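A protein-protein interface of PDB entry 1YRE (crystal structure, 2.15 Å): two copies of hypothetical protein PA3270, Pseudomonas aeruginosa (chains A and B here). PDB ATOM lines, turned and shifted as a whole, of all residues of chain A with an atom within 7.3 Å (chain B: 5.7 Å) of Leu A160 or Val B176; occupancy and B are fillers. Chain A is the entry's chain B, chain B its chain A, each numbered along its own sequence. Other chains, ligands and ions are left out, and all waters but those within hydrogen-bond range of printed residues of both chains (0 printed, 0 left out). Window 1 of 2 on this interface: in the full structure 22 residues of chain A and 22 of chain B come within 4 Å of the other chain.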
ATOM      1  N   GLN A 135       6.581  -9.152  -0.915  1.00  0.00           N
ATOM      2  CA  GLN A 135       7.017  -9.604   0.383  1.00  0.00           C
ATOM      3  C   GLN A 135       7.778  -8.453   1.121  1.00  0.00           C
ATOM      4  O   GLN A 135       8.459  -7.635   0.497  1.00  0.00           O
ATOM      5  CB  GLN A 135       7.976 -10.787   0.175  1.00  0.00           C
ATOM      6  CG  GLN A 135       8.742 -11.276   1.453  1.00  0.00           C
ATOM      7  CD  GLN A 135       9.425 -12.627   1.257  1.00  0.00           C
ATOM      8  OE1 GLN A 135       8.776 -13.613   0.846  1.00  0.00           O
ATOM      9  NE2 GLN A 135      10.715 -12.683   1.517  1.00  0.00           N
ATOM     10  N   SER A 137       9.960  -8.166   5.074  1.00  0.00           N
ATOM     11  CA  SER A 137      10.457  -8.942   6.170  1.00  0.00           C
ATOM     12  C   SER A 137      11.436  -8.090   7.034  1.00  0.00           C
ATOM     13  O   SER A 137      12.021  -7.103   6.565  1.00  0.00           O
ATOM     14  CB  SER A 137      11.118 -10.258   5.660  1.00  0.00           C
ATOM     15  OG  SER A 137      12.410  -9.971   5.184  1.00  0.00           O
ATOM     16  N   ALA A 140      13.030 -10.342  14.046  1.00  0.00           N
ATOM     17  CA  ALA A 140      12.139 -10.669  15.114  1.00  0.00           C
ATOM     18  C   ALA A 140      12.337  -9.654  16.246  1.00  0.00           C
ATOM     19  O   ALA A 140      11.371  -9.288  16.889  1.00  0.00           O
ATOM     20  CB  ALA A 140      12.410 -12.102  15.593  1.00  0.00           C
ATOM     21  N   GLU A 157       3.115 -13.690   7.566  1.00  0.00           N
ATOM     22  CA  GLU A 157       2.965 -15.018   6.946  1.00  0.00           C
ATOM     23  C   GLU A 157       3.719 -16.092   7.678  1.00  0.00           C
ATOM     24  O   GLU A 157       3.309 -17.253   7.634  1.00  0.00           O
ATOM     25  CB  GLU A 157       3.437 -14.992   5.478  1.00  0.00           C
ATOM     26  CG  GLU A 157       2.429 -14.300   4.555  1.00  0.00           C
ATOM     27  CD  GLU A 157       2.883 -14.227   3.131  1.00  0.00           C
ATOM     28  OE1 GLU A 157       4.098 -14.257   2.885  1.00  0.00           O
ATOM     29  OE2 GLU A 157       2.028 -14.111   2.234  1.00  0.00           O
ATOM     30  N   GLY A 158       4.827 -15.733   8.333  1.00  0.00           N
ATOM     31  CA  GLY A 158       5.565 -16.740   9.052  1.00  0.00           C
ATOM     32  C   GLY A 158       6.687 -16.189   9.852  1.00  0.00           C
ATOM     33  O   GLY A 158       6.935 -14.989   9.822  1.00  0.00           O
ATOM     34  N   VAL A 159       7.326 -17.057  10.619  1.00  0.00           N
ATOM     35  CA  VAL A 159       8.482 -16.711  11.381  1.00  0.00           C
ATOM     36  C   VAL A 159       9.542 -17.738  11.019  1.00  0.00           C
ATOM     37  O   VAL A 159       9.325 -18.965  11.242  1.00  0.00           O
ATOM     38  CB  VAL A 159       8.215 -16.834  12.909  1.00  0.00           C
ATOM     39  CG1 VAL A 159       9.492 -16.414  13.670  1.00  0.00           C
ATOM     40  CG2 VAL A 159       6.973 -16.037  13.287  1.00  0.00           C
ATOM     41  N   LEU A 160      10.668 -17.246  10.496  1.00  0.00           N
ATOM     42  CA  LEU A 160      11.749 -18.106  10.073  1.00  0.00           C
ATOM     43  C   LEU A 160      12.897 -18.059  11.059  1.00  0.00           C
ATOM     44  O   LEU A 160      13.373 -16.988  11.349  1.00  0.00           O
ATOM     45  CB  LEU A 160      12.212 -17.733   8.632  1.00  0.00           C
ATOM     46  CG  LEU A 160      11.158 -17.321   7.556  1.00  0.00           C
ATOM     47  CD1 LEU A 160      11.847 -16.819   6.274  1.00  0.00           C
ATOM     48  CD2 LEU A 160      10.159 -18.424   7.207  1.00  0.00           C
ATOM     49  N   ARG A 161      13.331 -19.229  11.572  1.00  0.00           N
ATOM     50  CA  ARG A 161      14.225 -19.325  12.720  1.00  0.00           C
ATOM     51  C   ARG A 161      15.654 -19.398  12.261  1.00  0.00           C
ATOM     52  O   ARG A 161      15.946 -20.001  11.207  1.00  0.00           O
ATOM     53  CB  ARG A 161      13.878 -20.557  13.558  1.00  0.00           C
ATOM     54  CG  ARG A 161      12.394 -20.671  13.893  1.00  0.00           C
ATOM     55  CD  ARG A 161      12.021 -22.007  14.532  1.00  0.00           C
ATOM     56  NE  ARG A 161      11.914 -23.118  13.567  1.00  0.00           N
ATOM     57  CZ  ARG A 161      12.159 -24.385  13.902  1.00  0.00           C
ATOM     58  NH1 ARG A 161      12.089 -25.360  13.010  1.00  0.00           N
ATOM     59  NH2 ARG A 161      12.513 -24.660  15.155  1.00  0.00           N
ATOM     60  N   ASN A 162      16.566 -18.771  13.005  1.00  0.00           N
ATOM     61  CA  ASN A 162      17.969 -18.804  12.624  1.00  0.00           C
ATOM     62  C   ASN A 162      18.153 -18.389  11.179  1.00  0.00           C
ATOM     63  O   ASN A 162      18.897 -19.049  10.431  1.00  0.00           O
ATOM     64  CB  ASN A 162      18.546 -20.219  12.814  1.00  0.00           C
ATOM     65  CG  ASN A 162      18.686 -20.593  14.285  1.00  0.00           C
ATOM     66  OD1 ASN A 162      18.147 -19.901  15.192  1.00  0.00           O
ATOM     67  ND2 ASN A 162      19.413 -21.661  14.539  1.00  0.00           N
ATOM     68  N   HIS A 163      17.504 -17.273  10.810  1.00  0.00           N
ATOM     69  CA  HIS A 163      17.384 -16.883   9.424  1.00  0.00           C
ATOM     70  C   HIS A 163      18.234 -15.608   9.080  1.00  0.00           C
ATOM     71  O   HIS A 163      18.416 -15.278   7.905  1.00  0.00           O
ATOM     72  CB  HIS A 163      15.895 -16.761   9.038  1.00  0.00           C
ATOM     73  CG  HIS A 163      15.689 -16.398   7.603  1.00  0.00           C
ATOM     74  ND1 HIS A 163      15.452 -15.109   7.192  1.00  0.00           N
ATOM     75  CD2 HIS A 163      15.746 -17.146   6.477  1.00  0.00           C
ATOM     76  CE1 HIS A 163      15.376 -15.078   5.877  1.00  0.00           C
ATOM     77  NE2 HIS A 163      15.522 -16.306   5.417  1.00  0.00           N
ATOM     78  N   ARG A 164      18.737 -14.932  10.121  1.00  0.00           N
ATOM     79  CA  ARG A 164      19.545 -13.747   9.966  1.00  0.00           C
ATOM     80  C   ARG A 164      20.524 -13.509  11.131  1.00  0.00           C
ATOM     81  O   ARG A 164      20.404 -14.099  12.227  1.00  0.00           O
ATOM     82  CB  ARG A 164      18.647 -12.505   9.819  1.00  0.00           C
ATOM     83  CG  ARG A 164      17.819 -12.220  11.071  1.00  0.00           C
ATOM     84  CD  ARG A 164      17.049 -10.893  10.942  1.00  0.00           C
ATOM     85  NE  ARG A 164      16.084 -10.914   9.848  1.00  0.00           N
ATOM     86  CZ  ARG A 164      15.955  -9.970   8.921  1.00  0.00           C
ATOM     87  NH1 ARG A 164      16.714  -8.896   8.924  1.00  0.00           N
ATOM     88  NH2 ARG A 164      15.028 -10.084   7.999  1.00  0.00           N
ATOM     89  N   ASP A 172      19.242 -14.149  14.716  1.00  0.00           N
ATOM     90  CA  ASP A 172      17.892 -13.776  15.020  1.00  0.00           C
ATOM     91  C   ASP A 172      16.983 -14.495  14.024  1.00  0.00           C
ATOM     92  O   ASP A 172      17.451 -15.065  13.044  1.00  0.00           O
ATOM     93  CB  ASP A 172      17.764 -12.239  14.932  1.00  0.00           C
ATOM     94  CG  ASP A 172      16.573 -11.698  15.671  1.00  0.00           C
ATOM     95  OD1 ASP A 172      15.910 -12.474  16.366  1.00  0.00           O
ATOM     96  OD2 ASP A 172      16.266 -10.470  15.555  1.00  0.00           O
ATOM     97  N   ASP A 173      15.700 -14.566  14.354  1.00  0.00           N
ATOM     98  CA  ASP A 173      14.659 -15.017  13.469  1.00  0.00           C
ATOM     99  C   ASP A 173      14.191 -13.853  12.557  1.00  0.00           C
ATOM    100  O   ASP A 173      14.617 -12.698  12.765  1.00  0.00           O
ATOM    101  CB  ASP A 173      13.467 -15.438  14.315  1.00  0.00           C
ATOM    102  CG  ASP A 173      13.748 -16.683  15.206  1.00  0.00           C
ATOM    103  OD1 ASP A 173      14.875 -17.283  15.167  1.00  0.00           O
ATOM    104  OD2 ASP A 173      12.793 -17.054  15.937  1.00  0.00           O
ATOM    105  N   THR A 174      13.272 -14.146  11.619  1.00  0.00           N
ATOM    106  CA  THR A 174      12.768 -13.192  10.618  1.00  0.00           C
ATOM    107  C   THR A 174      11.258 -13.304  10.620  1.00  0.00           C
ATOM    108  O   THR A 174      10.753 -14.414  10.601  1.00  0.00           O
ATOM    109  CB  THR A 174      13.381 -13.499   9.189  1.00  0.00           C
ATOM    110  OG1 THR A 174      14.751 -13.110   9.191  1.00  0.00           O
ATOM    111  CG2 THR A 174      12.705 -12.768   8.057  1.00  0.00           C
ATOM    112  N   PHE A 175      10.551 -12.182  10.757  1.00  0.00           N
ATOM    113  CA  PHE A 175       9.114 -12.135  10.464  1.00  0.00           C
ATOM    114  C   PHE A 175       8.906 -11.802   8.965  1.00  0.00           C
ATOM    115  O   PHE A 175       9.526 -10.869   8.426  1.00  0.00           O
ATOM    116  CB  PHE A 175       8.394 -11.099  11.328  1.00  0.00           C
ATOM    117  CG  PHE A 175       8.366 -11.427  12.858  1.00  0.00           C
ATOM    118  CD1 PHE A 175       8.908 -12.612  13.363  1.00  0.00           C
ATOM    119  CD2 PHE A 175       7.772 -10.527  13.756  1.00  0.00           C
ATOM    120  CE1 PHE A 175       8.904 -12.894  14.773  1.00  0.00           C
ATOM    121  CE2 PHE A 175       7.718 -10.808  15.203  1.00  0.00           C
ATOM    122  CZ  PHE A 175       8.282 -11.990  15.688  1.00  0.00           C
ATOM    123  N   VAL A 176       7.989 -12.536   8.315  1.00  0.00           N
ATOM    124  CA  VAL A 176       7.776 -12.463   6.866  1.00  0.00           C
ATOM    125  C   VAL A 176       6.312 -12.111   6.615  1.00  0.00           C
ATOM    126  O   VAL A 176       5.367 -12.687   7.260  1.00  0.00           O
ATOM    127  CB  VAL A 176       8.210 -13.771   6.156  1.00  0.00           C
ATOM    128  CG1 VAL A 176       8.117 -13.627   4.644  1.00  0.00           C
ATOM    129  CG2 VAL A 176       9.676 -14.016   6.484  1.00  0.00           C
ATOM    130  N   ARG B 133      20.600 -23.558  10.030  1.00  0.00           N
ATOM    131  CA  ARG B 133      19.198 -23.694   9.565  1.00  0.00           C
ATOM    132  C   ARG B 133      19.132 -24.450   8.244  1.00  0.00           C
ATOM    133  O   ARG B 133      19.982 -24.216   7.360  1.00  0.00           O
ATOM    134  CB  ARG B 133      18.559 -22.314   9.366  1.00  0.00           C
ATOM    135  CG  ARG B 133      17.379 -22.252   8.377  1.00  0.00           C
ATOM    136  CD  ARG B 133      16.854 -20.787   8.158  1.00  0.00           C
ATOM    137  NE  ARG B 133      15.668 -20.794   7.301  1.00  0.00           N
ATOM    138  CZ  ARG B 133      14.421 -20.988   7.736  1.00  0.00           C
ATOM    139  NH1 ARG B 133      13.412 -21.044   6.875  1.00  0.00           N
ATOM    140  NH2 ARG B 133      14.178 -21.113   9.029  1.00  0.00           N
ATOM    141  N   GLN B 135      16.038 -25.066   5.405  1.00  0.00           N
ATOM    142  CA  GLN B 135      14.665 -24.870   4.986  1.00  0.00           C
ATOM    143  C   GLN B 135      14.242 -25.949   3.983  1.00  0.00           C
ATOM    144  O   GLN B 135      15.052 -26.407   3.200  1.00  0.00           O
ATOM    145  CB  GLN B 135      14.525 -23.465   4.333  1.00  0.00           C
ATOM    146  CG  GLN B 135      13.175 -23.143   3.767  1.00  0.00           C
ATOM    147  CD  GLN B 135      13.104 -21.647   3.411  1.00  0.00           C
ATOM    148  OE1 GLN B 135      13.404 -20.794   4.238  1.00  0.00           O
ATOM    149  NE2 GLN B 135      12.741 -21.339   2.176  1.00  0.00           N
ATOM    150  N   LEU B 136      12.980 -26.332   4.036  1.00  0.00           N
ATOM    151  CA  LEU B 136      12.333 -27.213   3.063  1.00  0.00           C
ATOM    152  C   LEU B 136      11.001 -26.501   2.747  1.00  0.00           C
ATOM    153  O   LEU B 136      10.469 -25.858   3.651  1.00  0.00           O
ATOM    154  CB  LEU B 136      12.071 -28.583   3.730  1.00  0.00           C
ATOM    155  CG  LEU B 136      13.419 -29.226   4.180  1.00  0.00           C
ATOM    156  CD1 LEU B 136      13.459 -29.515   5.619  1.00  0.00           C
ATOM    157  CD2 LEU B 136      13.767 -30.489   3.367  1.00  0.00           C
ATOM    158  N   SER B 137      10.459 -26.631   1.517  1.00  0.00           N
ATOM    159  CA  SER B 137       9.258 -25.887   1.096  1.00  0.00           C
ATOM    160  C   SER B 137       8.476 -26.692   0.136  1.00  0.00           C
ATOM    161  O   SER B 137       9.052 -27.412  -0.590  1.00  0.00           O
ATOM    162  CB  SER B 137       9.659 -24.609   0.289  1.00  0.00           C
ATOM    163  OG  SER B 137      10.177 -23.712   1.206  1.00  0.00           O
ATOM    164  N   THR B 138       7.162 -26.484   0.066  1.00  0.00           N
ATOM    165  CA  THR B 138       6.375 -27.145  -0.962  1.00  0.00           C
ATOM    166  C   THR B 138       5.062 -26.402  -1.144  1.00  0.00           C
ATOM    167  O   THR B 138       4.663 -25.629  -0.271  1.00  0.00           O
ATOM    168  CB  THR B 138       6.137 -28.684  -0.583  1.00  0.00           C
ATOM    169  OG1 THR B 138       5.718 -29.401  -1.739  1.00  0.00           O
ATOM    170  CG2 THR B 138       5.098 -28.846   0.487  1.00  0.00           C
ATOM    171  N   GLN B 155       9.733 -28.424  11.160  1.00  0.00           N
ATOM    172  CA  GLN B 155       8.585 -27.687  11.787  1.00  0.00           C
ATOM    173  C   GLN B 155       8.071 -26.655  10.808  1.00  0.00           C
ATOM    174  O   GLN B 155       8.879 -25.978  10.227  1.00  0.00           O
ATOM    175  CB  GLN B 155       9.038 -26.968  13.077  1.00  0.00           C
ATOM    176  CG  GLN B 155       9.546 -27.925  14.233  1.00  0.00           C
ATOM    177  CD  GLN B 155       8.643 -29.196  14.489  1.00  0.00           C
ATOM    178  OE1 GLN B 155       7.408 -29.170  14.304  1.00  0.00           O
ATOM    179  NE2 GLN B 155       9.282 -30.303  14.919  1.00  0.00           N
ATOM    180  N   ARG B 156       6.749 -26.512  10.660  1.00  0.00           N
ATOM    181  CA  ARG B 156       6.195 -25.527   9.761  1.00  0.00           C
ATOM    182  C   ARG B 156       6.452 -24.094  10.278  1.00  0.00           C
ATOM    183  O   ARG B 156       6.268 -23.835  11.467  1.00  0.00           O
ATOM    184  CB  ARG B 156       4.711 -25.767   9.514  1.00  0.00           C
ATOM    185  CG  ARG B 156       4.328 -25.453   8.092  1.00  0.00           C
ATOM    186  CD  ARG B 156       3.236 -24.513   8.076  1.00  0.00           C
ATOM    187  NE  ARG B 156       1.973 -25.101   7.640  1.00  0.00           N
ATOM    188  CZ  ARG B 156       0.789 -24.604   7.980  1.00  0.00           C
ATOM    189  NH1 ARG B 156      -0.320 -25.176   7.533  1.00  0.00           N
ATOM    190  NH2 ARG B 156       0.715 -23.552   8.810  1.00  0.00           N
ATOM    191  N   GLU B 157       6.935 -23.199   9.403  1.00  0.00           N
ATOM    192  CA  GLU B 157       7.250 -21.838   9.828  1.00  0.00           C
ATOM    193  C   GLU B 157       6.321 -20.809   9.280  1.00  0.00           C
ATOM    194  O   GLU B 157       6.261 -19.721   9.814  1.00  0.00           O
ATOM    195  CB  GLU B 157       8.672 -21.440   9.427  1.00  0.00           C
ATOM    196  CG  GLU B 157       9.670 -22.075  10.264  1.00  0.00           C
ATOM    197  CD  GLU B 157      11.068 -21.735   9.897  1.00  0.00           C
ATOM    198  OE1 GLU B 157      11.368 -21.467   8.707  1.00  0.00           O
ATOM    199  OE2 GLU B 157      11.885 -21.796  10.839  1.00  0.00           O
ATOM    200  N   GLY B 158       5.657 -21.101   8.165  1.00  0.00           N
ATOM    201  CA  GLY B 158       4.849 -20.096   7.536  1.00  0.00           C
ATOM    202  C   GLY B 158       4.109 -20.558   6.322  1.00  0.00           C
ATOM    203  O   GLY B 158       4.411 -21.633   5.801  1.00  0.00           O
ATOM    204  N   VAL B 159       3.124 -19.756   5.904  1.00  0.00           N
ATOM    205  CA  VAL B 159       2.400 -19.919   4.628  1.00  0.00           C
ATOM    206  C   VAL B 159       2.547 -18.652   3.759  1.00  0.00           C
ATOM    207  O   VAL B 159       2.103 -17.580   4.145  1.00  0.00           O
ATOM    208  CB  VAL B 159       0.890 -20.157   4.845  1.00  0.00           C
ATOM    209  CG1 VAL B 159       0.270 -20.554   3.524  1.00  0.00           C
ATOM    210  CG2 VAL B 159       0.671 -21.305   5.901  1.00  0.00           C
ATOM    211  N   LEU B 160       3.209 -18.783   2.622  1.00  0.00           N
ATOM    212  CA  LEU B 160       3.554 -17.654   1.787  1.00  0.00           C
ATOM    213  C   LEU B 160       2.526 -17.619   0.694  1.00  0.00           C
ATOM    214  O   LEU B 160       2.464 -18.565  -0.036  1.00  0.00           O
ATOM    215  CB  LEU B 160       4.970 -17.845   1.190  1.00  0.00           C
ATOM    216  CG  LEU B 160       6.121 -18.048   2.200  1.00  0.00           C
ATOM    217  CD1 LEU B 160       7.468 -18.037   1.529  1.00  0.00           C
ATOM    218  CD2 LEU B 160       6.066 -17.017   3.341  1.00  0.00           C
ATOM    219  N   THR B 174       2.900 -21.314  -0.720  1.00  0.00           N
ATOM    220  CA  THR B 174       3.982 -22.209  -0.318  1.00  0.00           C
ATOM    221  C   THR B 174       3.893 -22.406   1.181  1.00  0.00           C
ATOM    222  O   THR B 174       3.667 -21.432   1.883  1.00  0.00           O
ATOM    223  CB  THR B 174       5.266 -21.559  -0.668  1.00  0.00           C
ATOM    224  OG1 THR B 174       5.371 -21.497  -2.124  1.00  0.00           O
ATOM    225  CG2 THR B 174       6.428 -22.316  -0.105  1.00  0.00           C
ATOM    226  N   PHE B 175       4.058 -23.654   1.654  1.00  0.00           N
ATOM    227  CA  PHE B 175       4.310 -23.977   3.075  1.00  0.00           C
ATOM    228  C   PHE B 175       5.801 -24.074   3.273  1.00  0.00           C
ATOM    229  O   PHE B 175       6.424 -24.856   2.637  1.00  0.00           O
ATOM    230  CB  PHE B 175       3.698 -25.352   3.446  1.00  0.00           C
ATOM    231  CG  PHE B 175       2.164 -25.378   3.541  1.00  0.00           C
ATOM    232  CD1 PHE B 175       1.392 -24.286   3.146  1.00  0.00           C
ATOM    233  CD2 PHE B 175       1.505 -26.535   3.988  1.00  0.00           C
ATOM    234  CE1 PHE B 175      -0.024 -24.311   3.175  1.00  0.00           C
ATOM    235  CE2 PHE B 175       0.068 -26.584   4.046  1.00  0.00           C
ATOM    236  CZ  PHE B 175      -0.684 -25.456   3.655  1.00  0.00           C
ATOM    237  N   VAL B 176       6.345 -23.292   4.191  1.00  0.00           N
ATOM    238  CA  VAL B 176       7.729 -23.228   4.527  1.00  0.00           C
ATOM    239  C   VAL B 176       7.990 -23.869   5.922  1.00  0.00           C
ATOM    240  O   VAL B 176       7.200 -23.648   6.880  1.00  0.00           O
ATOM    241  CB  VAL B 176       8.167 -21.743   4.562  1.00  0.00           C
ATOM    242  CG1 VAL B 176       9.607 -21.596   4.998  1.00  0.00           C
ATOM    243  CG2 VAL B 176       8.059 -21.178   3.193  1.00  0.00           C
ATOM    244  N   TYR B 177       9.095 -24.625   6.027  1.00  0.00           N
ATOM    245  CA  TYR B 177       9.438 -25.391   7.227  1.00  0.00           C
ATOM    246  C   TYR B 177      10.892 -25.218   7.438  1.00  0.00           C
ATOM    247  O   TYR B 177      11.595 -24.687   6.553  1.00  0.00           O
ATOM    248  CB  TYR B 177       9.312 -26.908   6.997  1.00  0.00           C
ATOM    249  CG  TYR B 177       7.980 -27.370   6.591  1.00  0.00           C
ATOM    250  CD1 TYR B 177       7.159 -28.064   7.484  1.00  0.00           C
ATOM    251  CD2 TYR B 177       7.523 -27.137   5.293  1.00  0.00           C
ATOM    252  CE1 TYR B 177       5.882 -28.476   7.074  1.00  0.00           C
ATOM    253  CE2 TYR B 177       6.299 -27.557   4.890  1.00  0.00           C
ATOM    254  CZ  TYR B 177       5.475 -28.237   5.804  1.00  0.00           C
ATOM    255  OH  TYR B 177       4.263 -28.662   5.348  1.00  0.00           O
ATOM    256  N   SER B 178      11.377 -25.685   8.591  1.00  0.00           N
ATOM    257  CA  SER B 178      12.840 -25.711   8.781  1.00  0.00           C
ATOM    258  C   SER B 178      13.310 -26.668   9.856  1.00  0.00           C
ATOM    259  O   SER B 178      12.550 -27.100  10.718  1.00  0.00           O
ATOM    260  CB  SER B 178      13.366 -24.322   9.139  1.00  0.00           C
ATOM    261  OG  SER B 178      13.005 -23.998  10.493  1.00  0.00           O
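N of Val A159 lies within hydrogen-bond range of O of Glu B157 (3.0 Å).
The backbone NH of Val B159 sits at hydrogen-bond distance from the backbone carbonyl oxygen of Glu A157 (3.0 Å).
O of Ser B178 sits at hydrogen-bond distance from NH1 of Arg A161.
NH2 of Arg B133 is in hydrogen-bond range of O of Arg A161 (3.0 Å).
OE2 of Glu B157 lies within salt-bridge range of NE of Arg A161, at 3.0 Å.
The guanidinium group (NH1) of Arg B133 is in hydrogen-bond range of the side-chain amide oxygen (OE1) of Gln B135, at 2.6 Å.
The backbone carbonyl oxygen (O) of Gln B155 sits at hydrogen-bond distance from the backbone NH (N) of Ser B178 (3.0 Å).
The side-chain carboxylate of Glu B157 lies within hydrogen-bond range of the side-chain hydroxyl of Ser B178 (2.5 Å).
OG of Ser B178 lies close to NH2 of Arg B133 (3.4 Å).
NH1 of Arg B133 lies within salt-bridge range of OE1 of Glu B157 (2.8 Å).
The backbone NH (N) of His A163 is in hydrogen-bond range of the backbone carbonyl oxygen (O) of Asp A172, at 3.1 Å.
Glu A157 touches Gly B158.
Glu A157 touches Leu B160 (OE1 to CD2, 3.4 Å).
Gly A158 touches Glu B157 (CA to O, 3.2 Å).
Gly B158 touches Gly A158 (CA to CA, 3.8 Å).
Arg B133 touches Leu A160.
Leu A160 touches Glu B157.
CD2 of Leu A160 touches CG1 of Val B176 (3.9 Å).
CB of Gln B155 touches NH1 of Arg A161, at 3.4 Å.
Asn A162 touches Arg B133 (O to CB, 3.5 Å).
NE of Arg B133 touches CD2 of His A163 (3.7 Å).
Leu A160 touches three residues of chain B.
Of the printed residues of chain B, His A163 touches Arg B133.
Of the printed residues of chain A, Gly B158 touches Glu A157 and Gly A158.
Printed residues of chain A within 4 Å of Val B176: Leu A160 (3.9 Å).
The nearest printed residue of chain A that does not touch Gly B158 is Val A159 (5.0 Å).
Of the 16 printed residues of chain B, 8 touch a printed residue of chain A.
Printed residues of chain B that touch a printed residue of chain A: Arg B133, Gln B155, Glu B157, Gly B158, Val B159, Leu B160, Val B176 and Ser B178.
Among the printed residues, 15 pairs touch across the chains.
Glu A157 touches Val B159, and with the chains exchanged Val A159 touches Glu B157.
Glu A157 touches Leu B160, and with the chains exchanged Leu A160 touches Glu B157.
Gly B158 touches its own counterpart, Gly A158.
Leu A160 touches Val B176, but with the chains exchanged Val A176 does not touch Leu B160 (4.2 Å).
Positions printed for both chains: 135, 137, 157, 158, 159, 160, 174, 175 and 176.
Of the 15 pairs that touch across the chains among the printed residues, 7 have their exchanged pair printed and touching as well.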
